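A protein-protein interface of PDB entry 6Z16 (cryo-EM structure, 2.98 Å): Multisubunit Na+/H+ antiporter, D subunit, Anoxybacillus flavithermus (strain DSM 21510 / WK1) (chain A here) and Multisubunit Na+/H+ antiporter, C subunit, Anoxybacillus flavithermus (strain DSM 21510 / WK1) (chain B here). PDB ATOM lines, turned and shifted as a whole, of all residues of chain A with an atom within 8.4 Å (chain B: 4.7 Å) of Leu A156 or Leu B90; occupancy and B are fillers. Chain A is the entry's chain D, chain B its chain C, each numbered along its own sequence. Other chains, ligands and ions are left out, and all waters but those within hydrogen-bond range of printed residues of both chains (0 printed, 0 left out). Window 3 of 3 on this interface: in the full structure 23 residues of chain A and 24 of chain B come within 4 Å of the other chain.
O of Ala B91 lies within hydrogen-bond range of OG of Ser B94, at 2.8 Å. The side-chain carboxylate (OE2) of Glu B97 is in salt-bridge range of the guanidinium group (NH2) of Arg B93 (2.4 Å). N of Gly A151 lies close to NE2 of Gln A155, at 3.4 Å.
Hydrophobic or aromatic side chains of chain A within 4 Å of the printed part of chain B: Tyr A144, Val A148, Leu A156 and Ile A160. Printed residues of chain B that touch a printed residue of chain A: Phe B86, Phe B87, Leu B90, Ser B94 and Glu B97. Hydrophobic or aromatic side chains of chain B that line the printed part of chain A: Phe B86, Phe B87 and Leu B90. Among the printed residues, no Asp or Glu carboxylate lies within 4 Å of a Lys or Arg side-chain nitrogen of the other chain.
The side-chain carboxylate (OE1) of Glu B97 sits close to the backbone carbonyl oxygen (O) of Gly A151, at 3.3 Å.
CB of Tyr A144 touches CE2 of Phe B86, 3.6 Å away. Phe B86 touches Val A148. CD1 of Leu B90 touches CG2 of Val A148, at 3.7 Å. Leu B90 touches Leu A156 (CD1 to CD2, 3.8 Å). Leu A156 touches Glu B97. Leu B90 touches Thr A159. O of Ile A160 touches CE1 of Phe B87, 3.9 Å away. Ile A160 touches Leu B90. CD1 of Ile A160 touches OG of Ser B94 (3.7 Å). CG2 of Thr A163 touches CD1 of Phe B87 (3.8 Å).
Of the printed residues of chain B, Tyr A144 touches Phe B86 (3.6 Å). Of the printed residues of chain B, Gly A151 touches Glu B97 (3.3 Å). Thr A152 touches none of the printed residues of chain B. Of the printed residues of chain B, Leu A156 touches Leu B90 and Glu B97. Of the printed residues of chain B, Thr A163 touches Phe B87 (3.8 Å). Leu A164 touches none of the printed residues of chain B. Printed residues of chain A within 4 Å of Phe B86: Tyr A144 (3.6 Å) and Val A148 (3.96 Å). Leu B90 touches just these residues of chain A: Val A148, Leu A156, Thr A159 and Ile A160. The nearest residue of chain B that does not touch Leu A156 is Arg B93 (4.2 Å).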
ATOM      1  N   TYR A 144      15.267  24.704  22.641  1.00  0.00           N
ATOM      2  CA  TYR A 144      16.351  24.702  21.651  1.00  0.00           C
ATOM      3  C   TYR A 144      17.598  25.353  22.217  1.00  0.00           C
ATOM      4  O   TYR A 144      18.710  24.818  22.102  1.00  0.00           O
ATOM      5  CB  TYR A 144      15.976  25.491  20.396  1.00  0.00           C
ATOM      6  CG  TYR A 144      14.810  25.056  19.561  1.00  0.00           C
ATOM      7  CD1 TYR A 144      14.328  23.757  19.571  1.00  0.00           C
ATOM      8  CD2 TYR A 144      14.162  25.988  18.774  1.00  0.00           C
ATOM      9  CE1 TYR A 144      13.228  23.412  18.798  1.00  0.00           C
ATOM     10  CE2 TYR A 144      13.084  25.659  18.017  1.00  0.00           C
ATOM     11  CZ  TYR A 144      12.618  24.381  18.026  1.00  0.00           C
ATOM     12  OH  TYR A 144      11.533  24.115  17.241  1.00  0.00           O
ATOM     13  N   VAL A 145      17.423  26.530  22.821  1.00  0.00           N
ATOM     14  CA  VAL A 145      18.592  27.278  23.268  1.00  0.00           C
ATOM     15  C   VAL A 145      19.215  26.621  24.497  1.00  0.00           C
ATOM     16  O   VAL A 145      20.444  26.532  24.605  1.00  0.00           O
ATOM     17  CB  VAL A 145      18.231  28.749  23.525  1.00  0.00           C
ATOM     18  CG1 VAL A 145      19.471  29.509  23.840  1.00  0.00           C
ATOM     19  CG2 VAL A 145      17.570  29.355  22.315  1.00  0.00           C
ATOM     20  N   LEU A 147      19.158  23.474  25.100  1.00  0.00           N
ATOM     21  CA  LEU A 147      19.844  22.295  24.593  1.00  0.00           C
ATOM     22  C   LEU A 147      21.198  22.648  23.993  1.00  0.00           C
ATOM     23  O   LEU A 147      22.172  21.912  24.177  1.00  0.00           O
ATOM     24  CB  LEU A 147      18.956  21.601  23.566  1.00  0.00           C
ATOM     25  CG  LEU A 147      19.439  20.332  22.878  1.00  0.00           C
ATOM     26  CD1 LEU A 147      19.703  19.257  23.880  1.00  0.00           C
ATOM     27  CD2 LEU A 147      18.387  19.872  21.909  1.00  0.00           C
ATOM     28  N   VAL A 148      21.291  23.774  23.279  1.00  0.00           N
ATOM     29  CA  VAL A 148      22.526  24.071  22.553  1.00  0.00           C
ATOM     30  C   VAL A 148      23.549  24.842  23.385  1.00  0.00           C
ATOM     31  O   VAL A 148      24.731  24.889  23.003  1.00  0.00           O
ATOM     32  CB  VAL A 148      22.184  24.828  21.251  1.00  0.00           C
ATOM     33  CG1 VAL A 148      21.816  26.273  21.528  1.00  0.00           C
ATOM     34  CG2 VAL A 148      23.283  24.686  20.190  1.00  0.00           C
ATOM     35  N   LEU A 149      23.150  25.399  24.529  1.00  0.00           N
ATOM     36  CA  LEU A 149      23.984  26.349  25.262  1.00  0.00           C
ATOM     37  C   LEU A 149      25.224  25.684  25.846  1.00  0.00           C
ATOM     38  O   LEU A 149      25.131  24.696  26.579  1.00  0.00           O
ATOM     39  CB  LEU A 149      23.165  27.009  26.371  1.00  0.00           C
ATOM     40  CG  LEU A 149      23.835  28.076  27.229  1.00  0.00           C
ATOM     41  CD1 LEU A 149      24.316  29.198  26.359  1.00  0.00           C
ATOM     42  CD2 LEU A 149      22.842  28.602  28.231  1.00  0.00           C
ATOM     43  N   GLY A 150      26.384  26.236  25.516  1.00  0.00           N
ATOM     44  CA  GLY A 150      27.654  25.646  25.882  1.00  0.00           C
ATOM     45  C   GLY A 150      28.462  25.305  24.652  1.00  0.00           C
ATOM     46  O   GLY A 150      29.667  25.559  24.597  1.00  0.00           O
ATOM     47  N   GLY A 151      27.792  24.737  23.654  1.00  0.00           N
ATOM     48  CA  GLY A 151      28.377  24.553  22.345  1.00  0.00           C
ATOM     49  C   GLY A 151      29.466  23.509  22.208  1.00  0.00           C
ATOM     50  O   GLY A 151      30.487  23.766  21.566  1.00  0.00           O
ATOM     51  N   THR A 152      29.276  22.336  22.798  1.00  0.00           N
ATOM     52  CA  THR A 152      30.119  21.202  22.455  1.00  0.00           C
ATOM     53  C   THR A 152      29.522  20.498  21.240  1.00  0.00           C
ATOM     54  O   THR A 152      28.435  20.839  20.775  1.00  0.00           O
ATOM     55  CB  THR A 152      30.267  20.246  23.640  1.00  0.00           C
ATOM     56  OG1 THR A 152      28.982  19.749  24.025  1.00  0.00           O
ATOM     57  CG2 THR A 152      30.889  20.957  24.821  1.00  0.00           C
ATOM     58  N   LYS A 153      30.245  19.497  20.726  1.00  0.00           N
ATOM     59  CA  LYS A 153      29.882  18.896  19.443  1.00  0.00           C
ATOM     60  C   LYS A 153      28.605  18.067  19.545  1.00  0.00           C
ATOM     61  O   LYS A 153      27.785  18.057  18.611  1.00  0.00           O
ATOM     62  CB  LYS A 153      31.043  18.046  18.942  1.00  0.00           C
ATOM     63  CG  LYS A 153      32.272  18.869  18.647  1.00  0.00           C
ATOM     64  CD  LYS A 153      33.415  18.025  18.148  1.00  0.00           C
ATOM     65  CE  LYS A 153      34.640  18.890  17.912  1.00  0.00           C
ATOM     66  NZ  LYS A 153      35.804  18.108  17.421  1.00  0.00           N
ATOM     67  N   ILE A 154      28.410  17.408  20.690  1.00  0.00           N
ATOM     68  CA  ILE A 154      27.278  16.510  20.875  1.00  0.00           C
ATOM     69  C   ILE A 154      25.975  17.294  20.885  1.00  0.00           C
ATOM     70  O   ILE A 154      25.024  16.963  20.165  1.00  0.00           O
ATOM     71  CB  ILE A 154      27.445  15.684  22.166  1.00  0.00           C
ATOM     72  CG1 ILE A 154      28.682  14.780  22.104  1.00  0.00           C
ATOM     73  CG2 ILE A 154      26.203  14.853  22.440  1.00  0.00           C
ATOM     74  CD1 ILE A 154      29.929  15.345  22.777  1.00  0.00           C
ATOM     75  N   GLN A 155      25.922  18.361  21.673  1.00  0.00           N
ATOM     76  CA  GLN A 155      24.693  19.134  21.736  1.00  0.00           C
ATOM     77  C   GLN A 155      24.469  19.991  20.497  1.00  0.00           C
ATOM     78  O   GLN A 155      23.314  20.274  20.189  1.00  0.00           O
ATOM     79  CB  GLN A 155      24.664  19.941  23.031  1.00  0.00           C
ATOM     80  CG  GLN A 155      25.918  20.691  23.354  1.00  0.00           C
ATOM     81  CD  GLN A 155      25.859  21.274  24.746  1.00  0.00           C
ATOM     82  OE1 GLN A 155      24.818  21.235  25.396  1.00  0.00           O
ATOM     83  NE2 GLN A 155      26.983  21.784  25.226  1.00  0.00           N
ATOM     84  N   LEU A 156      25.517  20.312  19.725  1.00  0.00           N
ATOM     85  CA  LEU A 156      25.312  20.858  18.380  1.00  0.00           C
ATOM     86  C   LEU A 156      24.565  19.878  17.481  1.00  0.00           C
ATOM     87  O   LEU A 156      23.544  20.239  16.870  1.00  0.00           O
ATOM     88  CB  LEU A 156      26.650  21.236  17.741  1.00  0.00           C
ATOM     89  CG  LEU A 156      27.333  22.531  18.163  1.00  0.00           C
ATOM     90  CD1 LEU A 156      28.701  22.606  17.540  1.00  0.00           C
ATOM     91  CD2 LEU A 156      26.496  23.715  17.749  1.00  0.00           C
ATOM     92  N   ARG A 157      25.061  18.631  17.399  1.00  0.00           N
ATOM     93  CA  ARG A 157      24.439  17.619  16.544  1.00  0.00           C
ATOM     94  C   ARG A 157      22.993  17.348  16.945  1.00  0.00           C
ATOM     95  O   ARG A 157      22.071  17.451  16.119  1.00  0.00           O
ATOM     96  CB  ARG A 157      25.242  16.321  16.586  1.00  0.00           C
ATOM     97  CG  ARG A 157      26.598  16.384  15.918  1.00  0.00           C
ATOM     98  CD  ARG A 157      27.157  14.988  15.692  1.00  0.00           C
ATOM     99  NE  ARG A 157      27.495  14.291  16.930  1.00  0.00           N
ATOM    100  CZ  ARG A 157      28.709  14.271  17.471  1.00  0.00           C
ATOM    101  NH1 ARG A 157      29.714  14.897  16.878  1.00  0.00           N
ATOM    102  NH2 ARG A 157      28.924  13.609  18.599  1.00  0.00           N
ATOM    103  N   GLU A 158      22.762  17.052  18.217  1.00  0.00           N
ATOM    104  CA  GLU A 158      21.389  16.735  18.565  1.00  0.00           C
ATOM    105  C   GLU A 158      20.493  17.959  18.708  1.00  0.00           C
ATOM    106  O   GLU A 158      19.269  17.799  18.646  1.00  0.00           O
ATOM    107  CB  GLU A 158      21.333  15.844  19.800  1.00  0.00           C
ATOM    108  CG  GLU A 158      21.498  14.365  19.404  1.00  0.00           C
ATOM    109  CD  GLU A 158      22.920  13.840  19.417  1.00  0.00           C
ATOM    110  OE1 GLU A 158      23.801  14.483  19.998  1.00  0.00           O
ATOM    111  OE2 GLU A 158      23.162  12.776  18.813  1.00  0.00           O
ATOM    112  N   THR A 159      21.044  19.176  18.771  1.00  0.00           N
ATOM    113  CA  THR A 159      20.195  20.350  18.621  1.00  0.00           C
ATOM    114  C   THR A 159      19.711  20.487  17.185  1.00  0.00           C
ATOM    115  O   THR A 159      18.553  20.859  16.956  1.00  0.00           O
ATOM    116  CB  THR A 159      20.941  21.609  19.059  1.00  0.00           C
ATOM    117  OG1 THR A 159      21.410  21.441  20.395  1.00  0.00           O
ATOM    118  CG2 THR A 159      20.012  22.805  19.047  1.00  0.00           C
ATOM    119  N   ILE A 160      20.575  20.159  16.211  1.00  0.00           N
ATOM    120  CA  ILE A 160      20.158  20.128  14.803  1.00  0.00           C
ATOM    121  C   ILE A 160      19.010  19.141  14.597  1.00  0.00           C
ATOM    122  O   ILE A 160      17.977  19.479  13.996  1.00  0.00           O
ATOM    123  CB  ILE A 160      21.356  19.798  13.897  1.00  0.00           C
ATOM    124  CG1 ILE A 160      22.357  20.946  13.893  1.00  0.00           C
ATOM    125  CG2 ILE A 160      20.908  19.496  12.493  1.00  0.00           C
ATOM    126  CD1 ILE A 160      23.626  20.634  13.172  1.00  0.00           C
ATOM    127  N   LYS A 161      19.154  17.933  15.160  1.00  0.00           N
ATOM    128  CA  LYS A 161      18.116  16.901  15.037  1.00  0.00           C
ATOM    129  C   LYS A 161      16.792  17.338  15.678  1.00  0.00           C
ATOM    130  O   LYS A 161      15.722  17.282  15.043  1.00  0.00           O
ATOM    131  CB  LYS A 161      18.591  15.604  15.690  1.00  0.00           C
ATOM    132  CG  LYS A 161      19.361  14.597  14.833  1.00  0.00           C
ATOM    133  CD  LYS A 161      20.721  15.104  14.396  1.00  0.00           C
ATOM    134  CE  LYS A 161      21.537  14.032  13.704  1.00  0.00           C
ATOM    135  NZ  LYS A 161      21.876  12.926  14.624  1.00  0.00           N
ATOM    136  N   TYR A 162      16.860  17.781  16.942  1.00  0.00           N
ATOM    137  CA  TYR A 162      15.680  18.172  17.709  1.00  0.00           C
ATOM    138  C   TYR A 162      14.964  19.362  17.076  1.00  0.00           C
ATOM    139  O   TYR A 162      13.721  19.387  16.996  1.00  0.00           O
ATOM    140  CB  TYR A 162      16.132  18.482  19.137  1.00  0.00           C
ATOM    141  CG  TYR A 162      15.076  18.942  20.102  1.00  0.00           C
ATOM    142  CD1 TYR A 162      14.136  18.062  20.599  1.00  0.00           C
ATOM    143  CD2 TYR A 162      15.056  20.247  20.562  1.00  0.00           C
ATOM    144  CE1 TYR A 162      13.179  18.477  21.500  1.00  0.00           C
ATOM    145  CE2 TYR A 162      14.107  20.671  21.460  1.00  0.00           C
ATOM    146  CZ  TYR A 162      13.169  19.780  21.924  1.00  0.00           C
ATOM    147  OH  TYR A 162      12.217  20.192  22.818  1.00  0.00           O
ATOM    148  N   THR A 163      15.739  20.330  16.572  1.00  0.00           N
ATOM    149  CA  THR A 163      15.175  21.522  15.955  1.00  0.00           C
ATOM    150  C   THR A 163      14.453  21.176  14.664  1.00  0.00           C
ATOM    151  O   THR A 163      13.358  21.692  14.408  1.00  0.00           O
ATOM    152  CB  THR A 163      16.285  22.533  15.684  1.00  0.00           C
ATOM    153  OG1 THR A 163      17.054  22.721  16.874  1.00  0.00           O
ATOM    154  CG2 THR A 163      15.694  23.861  15.282  1.00  0.00           C
ATOM    155  N   LEU A 164      15.045  20.277  13.867  1.00  0.00           N
ATOM    156  CA  LEU A 164      14.444  19.830  12.615  1.00  0.00           C
ATOM    157  C   LEU A 164      13.075  19.192  12.851  1.00  0.00           C
ATOM    158  O   LEU A 164      12.084  19.539  12.180  1.00  0.00           O
ATOM    159  CB  LEU A 164      15.408  18.843  11.960  1.00  0.00           C
ATOM    160  CG  LEU A 164      15.462  18.465  10.486  1.00  0.00           C
ATOM    161  CD1 LEU A 164      16.861  17.948  10.224  1.00  0.00           C
ATOM    162  CD2 LEU A 164      14.446  17.431  10.126  1.00  0.00           C
ATOM    163  N   ALA A 235      21.742  14.393  24.788  1.00  0.00           N
ATOM    164  CA  ALA A 235      22.576  15.595  24.673  1.00  0.00           C
ATOM    165  C   ALA A 235      22.710  16.526  25.895  1.00  0.00           C
ATOM    166  O   ALA A 235      23.852  16.798  26.284  1.00  0.00           O
ATOM    167  CB  ALA A 235      22.097  16.416  23.474  1.00  0.00           C
ATOM    168  N   PHE B  86      17.677  31.213  13.845  1.00  0.00           N
ATOM    169  CA  PHE B  86      18.393  30.401  14.827  1.00  0.00           C
ATOM    170  C   PHE B  86      18.990  29.145  14.203  1.00  0.00           C
ATOM    171  O   PHE B  86      20.155  28.813  14.450  1.00  0.00           O
ATOM    172  CB  PHE B  86      17.455  30.029  15.972  1.00  0.00           C
ATOM    173  CG  PHE B  86      18.057  29.071  16.956  1.00  0.00           C
ATOM    174  CD1 PHE B  86      19.023  29.491  17.852  1.00  0.00           C
ATOM    175  CD2 PHE B  86      17.650  27.746  16.985  1.00  0.00           C
ATOM    176  CE1 PHE B  86      19.577  28.604  18.754  1.00  0.00           C
ATOM    177  CE2 PHE B  86      18.206  26.858  17.874  1.00  0.00           C
ATOM    178  CZ  PHE B  86      19.169  27.287  18.760  1.00  0.00           C
ATOM    179  N   PHE B  87      18.217  28.458  13.363  1.00  0.00           N
ATOM    180  CA  PHE B  87      18.666  27.195  12.791  1.00  0.00           C
ATOM    181  C   PHE B  87      19.739  27.411  11.730  1.00  0.00           C
ATOM    182  O   PHE B  87      20.639  26.578  11.584  1.00  0.00           O
ATOM    183  CB  PHE B  87      17.433  26.448  12.276  1.00  0.00           C
ATOM    184  CG  PHE B  87      17.690  25.048  11.823  1.00  0.00           C
ATOM    185  CD1 PHE B  87      18.370  24.155  12.632  1.00  0.00           C
ATOM    186  CD2 PHE B  87      17.104  24.578  10.666  1.00  0.00           C
ATOM    187  CE1 PHE B  87      18.573  22.848  12.226  1.00  0.00           C
ATOM    188  CE2 PHE B  87      17.282  23.270  10.266  1.00  0.00           C
ATOM    189  CZ  PHE B  87      18.021  22.405  11.049  1.00  0.00           C
ATOM    190  N   LEU B  88      19.714  28.557  11.044  1.00  0.00           N
ATOM    191  CA  LEU B  88      20.783  28.886  10.104  1.00  0.00           C
ATOM    192  C   LEU B  88      22.088  29.221  10.815  1.00  0.00           C
ATOM    193  O   LEU B  88      23.163  28.793  10.371  1.00  0.00           O
ATOM    194  CB  LEU B  88      20.342  30.033   9.202  1.00  0.00           C
ATOM    195  CG  LEU B  88      19.389  29.603   8.095  1.00  0.00           C
ATOM    196  CD1 LEU B  88      18.697  30.786   7.474  1.00  0.00           C
ATOM    197  CD2 LEU B  88      20.211  28.876   7.052  1.00  0.00           C
ATOM    198  N   VAL B  89      22.022  29.968  11.925  1.00  0.00           N
ATOM    199  CA  VAL B  89      23.253  30.234  12.675  1.00  0.00           C
ATOM    200  C   VAL B  89      23.772  28.951  13.322  1.00  0.00           C
ATOM    201  O   VAL B  89      24.989  28.736  13.410  1.00  0.00           O
ATOM    202  CB  VAL B  89      23.023  31.360  13.706  1.00  0.00           C
ATOM    203  CG1 VAL B  89      24.276  31.647  14.515  1.00  0.00           C
ATOM    204  CG2 VAL B  89      22.594  32.625  13.003  1.00  0.00           C
ATOM    205  N   LEU B  90      22.864  28.048  13.710  1.00  0.00           N
ATOM    206  CA  LEU B  90      23.253  26.744  14.243  1.00  0.00           C
ATOM    207  C   LEU B  90      23.973  25.891  13.205  1.00  0.00           C
ATOM    208  O   LEU B  90      24.978  25.239  13.518  1.00  0.00           O
ATOM    209  CB  LEU B  90      22.009  26.024  14.750  1.00  0.00           C
ATOM    210  CG  LEU B  90      22.146  24.599  15.262  1.00  0.00           C
ATOM    211  CD1 LEU B  90      23.046  24.547  16.462  1.00  0.00           C
ATOM    212  CD2 LEU B  90      20.773  24.058  15.584  1.00  0.00           C
ATOM    213  N   ALA B  91      23.469  25.883  11.966  1.00  0.00           N
ATOM    214  CA  ALA B  91      24.142  25.176  10.880  1.00  0.00           C
ATOM    215  C   ALA B  91      25.508  25.780  10.582  1.00  0.00           C
ATOM    216  O   ALA B  91      26.463  25.054  10.278  1.00  0.00           O
ATOM    217  CB  ALA B  91      23.270  25.202   9.629  1.00  0.00           C
ATOM    218  N   TYR B  92      25.616  27.108  10.675  1.00  0.00           N
ATOM    219  CA  TYR B  92      26.907  27.776  10.521  1.00  0.00           C
ATOM    220  C   TYR B  92      27.895  27.351  11.604  1.00  0.00           C
ATOM    221  O   TYR B  92      29.073  27.093  11.318  1.00  0.00           O
ATOM    222  CB  TYR B  92      26.694  29.289  10.537  1.00  0.00           C
ATOM    223  CG  TYR B  92      27.958  30.106  10.458  1.00  0.00           C
ATOM    224  CD1 TYR B  92      28.673  30.202   9.274  1.00  0.00           C
ATOM    225  CD2 TYR B  92      28.424  30.803  11.563  1.00  0.00           C
ATOM    226  CE1 TYR B  92      29.829  30.954   9.201  1.00  0.00           C
ATOM    227  CE2 TYR B  92      29.578  31.554  11.500  1.00  0.00           C
ATOM    228  CZ  TYR B  92      30.275  31.627  10.316  1.00  0.00           C
ATOM    229  OH  TYR B  92      31.424  32.375  10.243  1.00  0.00           O
ATOM    230  N   ARG B  93      27.423  27.251  12.849  1.00  0.00           N
ATOM    231  CA  ARG B  93      28.276  26.815  13.952  1.00  0.00           C
ATOM    232  C   ARG B  93      28.731  25.373  13.776  1.00  0.00           C
ATOM    233  O   ARG B  93      29.892  25.039  14.053  1.00  0.00           O
ATOM    234  CB  ARG B  93      27.539  26.974  15.279  1.00  0.00           C
ATOM    235  CG  ARG B  93      27.277  28.401  15.675  1.00  0.00           C
ATOM    236  CD  ARG B  93      28.590  29.063  15.921  1.00  0.00           C
ATOM    237  NE  ARG B  93      29.280  28.387  17.006  1.00  0.00           N
ATOM    238  CZ  ARG B  93      30.589  28.426  17.184  1.00  0.00           C
ATOM    239  NH1 ARG B  93      31.347  29.098  16.336  1.00  0.00           N
ATOM    240  NH2 ARG B  93      31.137  27.784  18.200  1.00  0.00           N
ATOM    241  N   SER B  94      27.831  24.506  13.306  1.00  0.00           N
ATOM    242  CA  SER B  94      28.197  23.110  13.104  1.00  0.00           C
ATOM    243  C   SER B  94      29.150  22.936  11.929  1.00  0.00           C
ATOM    244  O   SER B  94      29.986  22.031  11.953  1.00  0.00           O
ATOM    245  CB  SER B  94      26.951  22.262  12.896  1.00  0.00           C
ATOM    246  OG  SER B  94      26.337  22.577  11.664  1.00  0.00           O
ATOM    247  N   GLU B  97      32.650  24.090  13.590  1.00  0.00           N
ATOM    248  CA  GLU B  97      33.344  23.278  14.587  1.00  0.00           C
ATOM    249  C   GLU B  97      33.486  21.809  14.201  1.00  0.00           C
ATOM    250  O   GLU B  97      34.553  21.224  14.410  1.00  0.00           O
ATOM    251  CB  GLU B  97      32.654  23.392  15.947  1.00  0.00           C
ATOM    252  CG  GLU B  97      32.886  24.742  16.605  1.00  0.00           C
ATOM    253  CD  GLU B  97      32.316  24.828  18.000  1.00  0.00           C
ATOM    254  OE1 GLU B  97      31.645  23.868  18.432  1.00  0.00           O
ATOM    255  OE2 GLU B  97      32.540  25.862  18.666  1.00  0.00           O
